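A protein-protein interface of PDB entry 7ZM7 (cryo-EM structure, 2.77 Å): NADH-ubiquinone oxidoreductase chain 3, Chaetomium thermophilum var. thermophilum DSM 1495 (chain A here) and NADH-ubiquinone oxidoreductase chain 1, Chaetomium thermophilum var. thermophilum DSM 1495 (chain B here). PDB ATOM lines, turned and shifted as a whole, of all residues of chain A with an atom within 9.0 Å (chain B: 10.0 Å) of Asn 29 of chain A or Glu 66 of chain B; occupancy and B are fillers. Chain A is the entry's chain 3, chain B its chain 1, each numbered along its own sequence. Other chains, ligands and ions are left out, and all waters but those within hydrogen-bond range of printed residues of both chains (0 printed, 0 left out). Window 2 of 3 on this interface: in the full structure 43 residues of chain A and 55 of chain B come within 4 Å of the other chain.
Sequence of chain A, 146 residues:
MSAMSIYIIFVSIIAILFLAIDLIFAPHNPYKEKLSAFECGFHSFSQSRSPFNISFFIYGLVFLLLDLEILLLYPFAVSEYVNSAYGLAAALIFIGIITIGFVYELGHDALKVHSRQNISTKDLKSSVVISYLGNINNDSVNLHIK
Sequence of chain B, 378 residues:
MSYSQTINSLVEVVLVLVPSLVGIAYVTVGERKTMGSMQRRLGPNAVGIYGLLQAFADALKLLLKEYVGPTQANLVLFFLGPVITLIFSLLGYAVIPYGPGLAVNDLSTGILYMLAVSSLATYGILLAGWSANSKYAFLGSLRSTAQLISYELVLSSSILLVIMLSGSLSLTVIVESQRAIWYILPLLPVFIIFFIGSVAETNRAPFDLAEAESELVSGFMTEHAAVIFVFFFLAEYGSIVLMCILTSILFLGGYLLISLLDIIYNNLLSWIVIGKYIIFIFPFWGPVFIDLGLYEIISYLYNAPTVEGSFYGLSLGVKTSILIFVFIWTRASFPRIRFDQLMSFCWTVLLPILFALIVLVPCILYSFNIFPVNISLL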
ATOM      1  N   ASP A  22     -24.222  11.165 -10.064  1.00  0.00           N
ATOM      2  CA  ASP A  22     -24.445  12.599 -10.191  1.00  0.00           C
ATOM      3  C   ASP A  22     -24.760  13.243  -8.845  1.00  0.00           C
ATOM      4  O   ASP A  22     -24.147  14.239  -8.464  1.00  0.00           O
ATOM      5  CB  ASP A  22     -25.569  12.860 -11.186  1.00  0.00           C
ATOM      6  CG  ASP A  22     -26.050  14.288 -11.146  1.00  0.00           C
ATOM      7  OD1 ASP A  22     -25.202  15.195 -11.117  1.00  0.00           O
ATOM      8  OD2 ASP A  22     -27.277  14.508 -11.139  1.00  0.00           O
ATOM      9  N   PHE A  25     -21.571  12.463  -6.355  1.00  0.00           N
ATOM     10  CA  PHE A  25     -20.211  12.868  -6.681  1.00  0.00           C
ATOM     11  C   PHE A  25     -20.104  14.231  -7.339  1.00  0.00           C
ATOM     12  O   PHE A  25     -19.097  14.916  -7.140  1.00  0.00           O
ATOM     13  CB  PHE A  25     -19.556  11.824  -7.592  1.00  0.00           C
ATOM     14  CG  PHE A  25     -18.988  10.655  -6.852  1.00  0.00           C
ATOM     15  CD1 PHE A  25     -18.235  10.847  -5.704  1.00  0.00           C
ATOM     16  CD2 PHE A  25     -19.199   9.368  -7.299  1.00  0.00           C
ATOM     17  CE1 PHE A  25     -17.705   9.777  -5.019  1.00  0.00           C
ATOM     18  CE2 PHE A  25     -18.673   8.292  -6.618  1.00  0.00           C
ATOM     19  CZ  PHE A  25     -17.925   8.497  -5.476  1.00  0.00           C
ATOM     20  N   ALA A  26     -21.086  14.632  -8.136  1.00  0.00           N
ATOM     21  CA  ALA A  26     -21.047  15.945  -8.743  1.00  0.00           C
ATOM     22  C   ALA A  26     -21.253  17.016  -7.674  1.00  0.00           C
ATOM     23  O   ALA A  26     -22.004  16.815  -6.720  1.00  0.00           O
ATOM     24  CB  ALA A  26     -22.111  16.064  -9.826  1.00  0.00           C
ATOM     25  N   PRO A  27     -20.567  18.145  -7.788  1.00  0.00           N
ATOM     26  CA  PRO A  27     -20.790  19.235  -6.839  1.00  0.00           C
ATOM     27  C   PRO A  27     -22.182  19.817  -6.975  1.00  0.00           C
ATOM     28  O   PRO A  27     -22.821  19.729  -8.024  1.00  0.00           O
ATOM     29  CB  PRO A  27     -19.717  20.257  -7.216  1.00  0.00           C
ATOM     30  CG  PRO A  27     -18.671  19.462  -7.870  1.00  0.00           C
ATOM     31  CD  PRO A  27     -19.389  18.391  -8.626  1.00  0.00           C
ATOM     32  N   HIS A  28     -22.659  20.403  -5.878  1.00  0.00           N
ATOM     33  CA  HIS A  28     -24.029  20.899  -5.778  1.00  0.00           C
ATOM     34  C   HIS A  28     -24.032  22.274  -5.114  1.00  0.00           C
ATOM     35  O   HIS A  28     -24.055  22.383  -3.886  1.00  0.00           O
ATOM     36  CB  HIS A  28     -24.887  19.905  -5.021  1.00  0.00           C
ATOM     37  CG  HIS A  28     -25.177  18.658  -5.787  1.00  0.00           C
ATOM     38  ND1 HIS A  28     -24.378  17.539  -5.724  1.00  0.00           N
ATOM     39  CD2 HIS A  28     -26.192  18.348  -6.624  1.00  0.00           C
ATOM     40  CE1 HIS A  28     -24.879  16.599  -6.504  1.00  0.00           C
ATOM     41  NE2 HIS A  28     -25.986  17.061  -7.054  1.00  0.00           N
ATOM     42  N   ASN A  29     -24.013  23.322  -5.920  1.00  0.00           N
ATOM     43  CA  ASN A  29     -24.143  24.669  -5.377  1.00  0.00           C
ATOM     44  C   ASN A  29     -25.592  24.931  -4.991  1.00  0.00           C
ATOM     45  O   ASN A  29     -26.494  24.725  -5.812  1.00  0.00           O
ATOM     46  CB  ASN A  29     -23.673  25.712  -6.382  1.00  0.00           C
ATOM     47  CG  ASN A  29     -22.181  25.917  -6.344  1.00  0.00           C
ATOM     48  OD1 ASN A  29     -21.494  25.389  -5.472  1.00  0.00           O
ATOM     49  ND2 ASN A  29     -21.667  26.692  -7.289  1.00  0.00           N
ATOM     50  N   PRO A  30     -25.860  25.369  -3.760  1.00  0.00           N
ATOM     51  CA  PRO A  30     -27.256  25.604  -3.359  1.00  0.00           C
ATOM     52  C   PRO A  30     -27.953  26.652  -4.202  1.00  0.00           C
ATOM     53  O   PRO A  30     -29.159  26.541  -4.450  1.00  0.00           O
ATOM     54  CB  PRO A  30     -27.126  26.052  -1.898  1.00  0.00           C
ATOM     55  CG  PRO A  30     -25.740  26.596  -1.791  1.00  0.00           C
ATOM     56  CD  PRO A  30     -24.904  25.762  -2.713  1.00  0.00           C
ATOM     57  N   TYR A  31     -27.223  27.668  -4.656  1.00  0.00           N
ATOM     58  CA  TYR A  31     -27.839  28.759  -5.394  1.00  0.00           C
ATOM     59  C   TYR A  31     -28.401  28.262  -6.720  1.00  0.00           C
ATOM     60  O   TYR A  31     -27.652  27.938  -7.645  1.00  0.00           O
ATOM     61  CB  TYR A  31     -26.819  29.872  -5.632  1.00  0.00           C
ATOM     62  N   LYS A  32     -29.727  28.214  -6.809  1.00  0.00           N
ATOM     63  CA  LYS A  32     -30.416  27.781  -8.016  1.00  0.00           C
ATOM     64  C   LYS A  32     -30.898  28.952  -8.859  1.00  0.00           C
ATOM     65  O   LYS A  32     -31.642  28.746  -9.822  1.00  0.00           O
ATOM     66  CB  LYS A  32     -31.595  26.876  -7.654  1.00  0.00           C
ATOM     67  N   GLU A  33     -30.497  30.171  -8.521  1.00  0.00           N
ATOM     68  CA  GLU A  33     -30.930  31.347  -9.262  1.00  0.00           C
ATOM     69  C   GLU A  33     -30.262  31.429 -10.632  1.00  0.00           C
ATOM     70  O   GLU A  33     -29.650  32.439 -10.972  1.00  0.00           O
ATOM     71  CB  GLU A  33     -30.635  32.610  -8.464  1.00  0.00           C
ATOM     72  N   LEU B  60     -18.046   9.679 -18.004  1.00  0.00           N
ATOM     73  CA  LEU B  60     -17.693   9.910 -16.577  1.00  0.00           C
ATOM     74  C   LEU B  60     -17.528  11.414 -16.338  1.00  0.00           C
ATOM     75  O   LEU B  60     -17.782  11.861 -15.223  1.00  0.00           O
ATOM     76  CB  LEU B  60     -16.416   9.134 -16.246  1.00  0.00           C
ATOM     77  CG  LEU B  60     -15.902   9.296 -14.817  1.00  0.00           C
ATOM     78  CD1 LEU B  60     -16.871   8.685 -13.817  1.00  0.00           C
ATOM     79  CD2 LEU B  60     -14.521   8.687 -14.671  1.00  0.00           C
ATOM     80  N   LYS B  61     -17.067  12.151 -17.392  1.00  0.00           N
ATOM     81  CA  LYS B  61     -16.930  13.615 -17.214  1.00  0.00           C
ATOM     82  C   LYS B  61     -18.315  14.198 -16.982  1.00  0.00           C
ATOM     83  O   LYS B  61     -18.465  14.978 -16.032  1.00  0.00           O
ATOM     84  CB  LYS B  61     -16.347  14.292 -18.449  1.00  0.00           C
ATOM     85  CG  LYS B  61     -15.940  15.737 -18.213  1.00  0.00           C
ATOM     86  CD  LYS B  61     -16.003  16.564 -19.453  1.00  0.00           C
ATOM     87  CE  LYS B  61     -17.369  16.561 -20.099  1.00  0.00           C
ATOM     88  NZ  LYS B  61     -17.362  17.383 -21.328  1.00  0.00           N
ATOM     89  N   LEU B  62     -19.276  13.843 -17.836  1.00  0.00           N
ATOM     90  CA  LEU B  62     -20.588  14.439 -17.664  1.00  0.00           C
ATOM     91  C   LEU B  62     -21.180  14.082 -16.314  1.00  0.00           C
ATOM     92  O   LEU B  62     -21.803  14.924 -15.662  1.00  0.00           O
ATOM     93  CB  LEU B  62     -21.519  13.999 -18.788  1.00  0.00           C
ATOM     94  CG  LEU B  62     -21.303  14.632 -20.156  1.00  0.00           C
ATOM     95  CD1 LEU B  62     -22.340  14.127 -21.111  1.00  0.00           C
ATOM     96  CD2 LEU B  62     -21.355  16.129 -20.065  1.00  0.00           C
ATOM     97  N   LEU B  63     -20.988  12.841 -15.872  1.00  0.00           N
ATOM     98  CA  LEU B  63     -21.545  12.414 -14.599  1.00  0.00           C
ATOM     99  C   LEU B  63     -21.035  13.264 -13.446  1.00  0.00           C
ATOM    100  O   LEU B  63     -21.776  13.529 -12.495  1.00  0.00           O
ATOM    101  CB  LEU B  63     -21.210  10.946 -14.357  1.00  0.00           C
ATOM    102  CG  LEU B  63     -22.139   9.887 -14.945  1.00  0.00           C
ATOM    103  CD1 LEU B  63     -21.608   8.527 -14.631  1.00  0.00           C
ATOM    104  CD2 LEU B  63     -23.540  10.041 -14.436  1.00  0.00           C
ATOM    105  N   LEU B  64     -19.778  13.686 -13.504  1.00  0.00           N
ATOM    106  CA  LEU B  64     -19.156  14.466 -12.446  1.00  0.00           C
ATOM    107  C   LEU B  64     -19.406  15.952 -12.578  1.00  0.00           C
ATOM    108  O   LEU B  64     -18.973  16.715 -11.716  1.00  0.00           O
ATOM    109  CB  LEU B  64     -17.650  14.219 -12.422  1.00  0.00           C
ATOM    110  CG  LEU B  64     -17.167  12.787 -12.252  1.00  0.00           C
ATOM    111  CD1 LEU B  64     -15.675  12.790 -12.253  1.00  0.00           C
ATOM    112  CD2 LEU B  64     -17.665  12.220 -10.990  1.00  0.00           C
ATOM    113  N   LYS B  65     -20.066  16.381 -13.637  1.00  0.00           N
ATOM    114  CA  LYS B  65     -20.290  17.792 -13.865  1.00  0.00           C
ATOM    115  C   LYS B  65     -21.398  18.316 -12.969  1.00  0.00           C
ATOM    116  O   LYS B  65     -22.355  17.616 -12.644  1.00  0.00           O
ATOM    117  CB  LYS B  65     -20.646  18.045 -15.322  1.00  0.00           C
ATOM    118  CG  LYS B  65     -20.573  19.481 -15.712  1.00  0.00           C
ATOM    119  CD  LYS B  65     -20.615  19.656 -17.209  1.00  0.00           C
ATOM    120  CE  LYS B  65     -20.524  21.127 -17.568  1.00  0.00           C
ATOM    121  NZ  LYS B  65     -19.358  21.788 -16.915  1.00  0.00           N
ATOM    122  N   GLU B  66     -21.258  19.572 -12.573  1.00  0.00           N
ATOM    123  CA  GLU B  66     -22.343  20.262 -11.910  1.00  0.00           C
ATOM    124  C   GLU B  66     -23.521  20.434 -12.856  1.00  0.00           C
ATOM    125  O   GLU B  66     -23.374  20.566 -14.071  1.00  0.00           O
ATOM    126  CB  GLU B  66     -21.879  21.623 -11.408  1.00  0.00           C
ATOM    127  CG  GLU B  66     -22.920  22.385 -10.630  1.00  0.00           C
ATOM    128  CD  GLU B  66     -22.492  23.789 -10.345  1.00  0.00           C
ATOM    129  OE1 GLU B  66     -23.364  24.644 -10.081  1.00  0.00           O
ATOM    130  OE2 GLU B  66     -21.279  24.046 -10.383  1.00  0.00           O
ATOM    131  N   TYR B  67     -24.710  20.413 -12.281  1.00  0.00           N
ATOM    132  CA  TYR B  67     -25.945  20.648 -13.014  1.00  0.00           C
ATOM    133  C   TYR B  67     -26.680  21.774 -12.314  1.00  0.00           C
ATOM    134  O   TYR B  67     -26.906  21.720 -11.105  1.00  0.00           O
ATOM    135  CB  TYR B  67     -26.770  19.365 -13.116  1.00  0.00           C
ATOM    136  CG  TYR B  67     -27.218  18.839 -11.785  1.00  0.00           C
ATOM    137  CD1 TYR B  67     -26.421  17.958 -11.083  1.00  0.00           C
ATOM    138  CD2 TYR B  67     -28.432  19.202 -11.240  1.00  0.00           C
ATOM    139  CE1 TYR B  67     -26.807  17.475  -9.870  1.00  0.00           C
ATOM    140  CE2 TYR B  67     -28.829  18.729 -10.018  1.00  0.00           C
ATOM    141  CZ  TYR B  67     -28.018  17.862  -9.337  1.00  0.00           C
ATOM    142  OH  TYR B  67     -28.427  17.377  -8.120  1.00  0.00           O
ATOM    143  N   VAL B  68     -27.001  22.814 -13.068  1.00  0.00           N
ATOM    144  CA  VAL B  68     -27.565  24.029 -12.520  1.00  0.00           C
ATOM    145  C   VAL B  68     -28.978  24.261 -13.055  1.00  0.00           C
ATOM    146  O   VAL B  68     -29.521  25.359 -12.936  1.00  0.00           O
ATOM    147  CB  VAL B  68     -26.646  25.230 -12.794  1.00  0.00           C
ATOM    148  CG1 VAL B  68     -26.596  25.543 -14.284  1.00  0.00           C
ATOM    149  CG2 VAL B  68     -27.005  26.450 -11.939  1.00  0.00           C
ATOM    150  N   GLY B  69     -29.581  23.237 -13.647  1.00  0.00           N
ATOM    151  CA  GLY B  69     -30.915  23.347 -14.182  1.00  0.00           C
ATOM    152  C   GLY B  69     -31.906  23.715 -13.102  1.00  0.00           C
ATOM    153  O   GLY B  69     -31.659  23.524 -11.907  1.00  0.00           O
ATOM    154  N   THR B  71     -34.373  23.592 -10.392  1.00  0.00           N
ATOM    155  CA  THR B  71     -35.008  22.669  -9.467  1.00  0.00           C
ATOM    156  C   THR B  71     -36.250  23.261  -8.816  1.00  0.00           C
ATOM    157  O   THR B  71     -36.907  22.573  -8.027  1.00  0.00           O
ATOM    158  CB  THR B  71     -34.017  22.237  -8.382  1.00  0.00           C
ATOM    159  N   PHE B  79     -35.414  15.815 -12.198  1.00  0.00           N
ATOM    160  CA  PHE B  79     -34.636  14.630 -11.855  1.00  0.00           C
ATOM    161  C   PHE B  79     -35.231  13.336 -12.392  1.00  0.00           C
ATOM    162  O   PHE B  79     -34.517  12.549 -13.021  1.00  0.00           O
ATOM    163  CB  PHE B  79     -34.481  14.523 -10.340  1.00  0.00           C
ATOM    164  CG  PHE B  79     -33.418  15.410  -9.788  1.00  0.00           C
ATOM    165  CD1 PHE B  79     -33.697  16.724  -9.468  1.00  0.00           C
ATOM    166  CD2 PHE B  79     -32.139  14.932  -9.593  1.00  0.00           C
ATOM    167  CE1 PHE B  79     -32.718  17.545  -8.958  1.00  0.00           C
ATOM    168  CE2 PHE B  79     -31.159  15.747  -9.087  1.00  0.00           C
ATOM    169  CZ  PHE B  79     -31.449  17.056  -8.766  1.00  0.00           C
ATOM    170  N   HIS B 224     -29.386  26.179 -22.394  1.00  0.00           N
ATOM    171  CA  HIS B 224     -30.067  24.896 -22.516  1.00  0.00           C
ATOM    172  C   HIS B 224     -30.091  24.146 -21.186  1.00  0.00           C
ATOM    173  O   HIS B 224     -29.663  24.650 -20.144  1.00  0.00           O
ATOM    174  CB  HIS B 224     -29.389  24.033 -23.580  1.00  0.00           C
ATOM    175  N   ALA B 225     -30.615  22.920 -21.235  1.00  0.00           N
ATOM    176  CA  ALA B 225     -30.745  22.067 -20.059  1.00  0.00           C
ATOM    177  C   ALA B 225     -30.118  20.690 -20.239  1.00  0.00           C
ATOM    178  O   ALA B 225     -29.763  20.053 -19.242  1.00  0.00           O
ATOM    179  CB  ALA B 225     -32.221  21.909 -19.685  1.00  0.00           C
ATOM    180  N   ALA B 226     -30.087  20.195 -21.485  1.00  0.00           N
ATOM    181  CA  ALA B 226     -29.356  18.938 -21.771  1.00  0.00           C
ATOM    182  C   ALA B 226     -27.894  19.347 -21.668  1.00  0.00           C
ATOM    183  O   ALA B 226     -27.321  19.736 -22.702  1.00  0.00           O
ATOM    184  CB  ALA B 226     -29.699  18.443 -23.154  1.00  0.00           C
ATOM    185  N   VAL B 227     -27.314  19.255 -20.472  1.00  0.00           N
ATOM    186  CA  VAL B 227     -25.994  19.825 -20.246  1.00  0.00           C
ATOM    187  C   VAL B 227     -25.038  18.805 -19.659  1.00  0.00           C
ATOM    188  O   VAL B 227     -23.994  18.498 -20.250  1.00  0.00           O
ATOM    189  CB  VAL B 227     -26.091  21.045 -19.321  1.00  0.00           C
ATOM    190  N   ILE B 228     -25.369  18.297 -18.476  1.00  0.00           N
ATOM    191  CA  ILE B 228     -24.496  17.372 -17.770  1.00  0.00           C
ATOM    192  C   ILE B 228     -25.058  15.960 -17.866  1.00  0.00           C
ATOM    193  O   ILE B 228     -24.483  15.013 -17.320  1.00  0.00           O
ATOM    194  CB  ILE B 228     -24.318  17.808 -16.308  1.00  0.00           C
ATOM    195  N   PHE B 229     -26.178  15.810 -18.579  1.00  0.00           N
ATOM    196  CA  PHE B 229     -26.924  14.552 -18.606  1.00  0.00           C
ATOM    197  C   PHE B 229     -26.444  13.648 -19.734  1.00  0.00           C
ATOM    198  O   PHE B 229     -26.512  14.005 -20.915  1.00  0.00           O
ATOM    199  CB  PHE B 229     -28.417  14.813 -18.730  1.00  0.00           C
ATOM    200  CG  PHE B 229     -28.968  15.648 -17.627  1.00  0.00           C
ATOM    201  CD1 PHE B 229     -28.850  15.233 -16.316  1.00  0.00           C
ATOM    202  CD2 PHE B 229     -29.605  16.845 -17.892  1.00  0.00           C
ATOM    203  CE1 PHE B 229     -29.352  15.985 -15.293  1.00  0.00           C
ATOM    204  CE2 PHE B 229     -30.111  17.609 -16.868  1.00  0.00           C
ATOM    205  CZ  PHE B 229     -29.983  17.179 -15.564  1.00  0.00           C
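OH of Tyr 67 of chain B lies within hydrogen-bond range of NE2 of His 28 of chain A (2.7 Å).
The backbone carbonyl oxygen (O) of Ala 26 of chain A is in hydrogen-bond range of a ring nitrogen (ND1) of His 28 of chain A (2.7 Å).
Among the printed residues, merely in contact across the chains: Asp 22 of chain A with Tyr 67 of chain B, Ala 26 of chain A with Lys 65 of chain B, Pro 27 of chain A with Leu 64 of chain B, Asp 22 of chain A with Leu 63 of chain B, Ala 26 of chain A with Leu 63 of chain B, Ala 26 of chain A with Leu 64 of chain B, Pro 27 of chain A with Glu 66 of chain B, Asn 29 of chain A with Glu 66 of chain B and Phe 25 of chain A with Leu 64 of chain B.
Asn 29 of chain A touches just one residue of chain B: Glu 66 (3.9 Å). Glu 66 of chain B touches just these residues of chain A: Pro 27 (3.7 Å) and Asn 29 (3.9 Å). Pro 27 of chain A touches two residues of chain B. No residue of chain B comes within 4 Å of Pro 30 of chain A. No residue of chain B comes within 4 Å of Tyr 31 of chain A. Of the printed residues of chain B, Ala 26 of chain A touches Leu 63, Leu 64 and Lys 65. Of the printed residues of chain A, Leu 63 of chain B touches Asp 22 (3.6 Å) and Ala 26 (3.7 Å). The nearest residue of chain A that does not touch Glu 66 of chain B is Ala 26 of chain A (4.5 Å).
Of the 10 printed residues of chain A, 6 touch a printed residue of chain B. Hydrophobic or aromatic side chains of chain A within 4 Å of the printed part of chain B: Phe 25, Ala 26, Pro 27 and His 28. Among the printed residues, 10 pairs touch across the chains.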
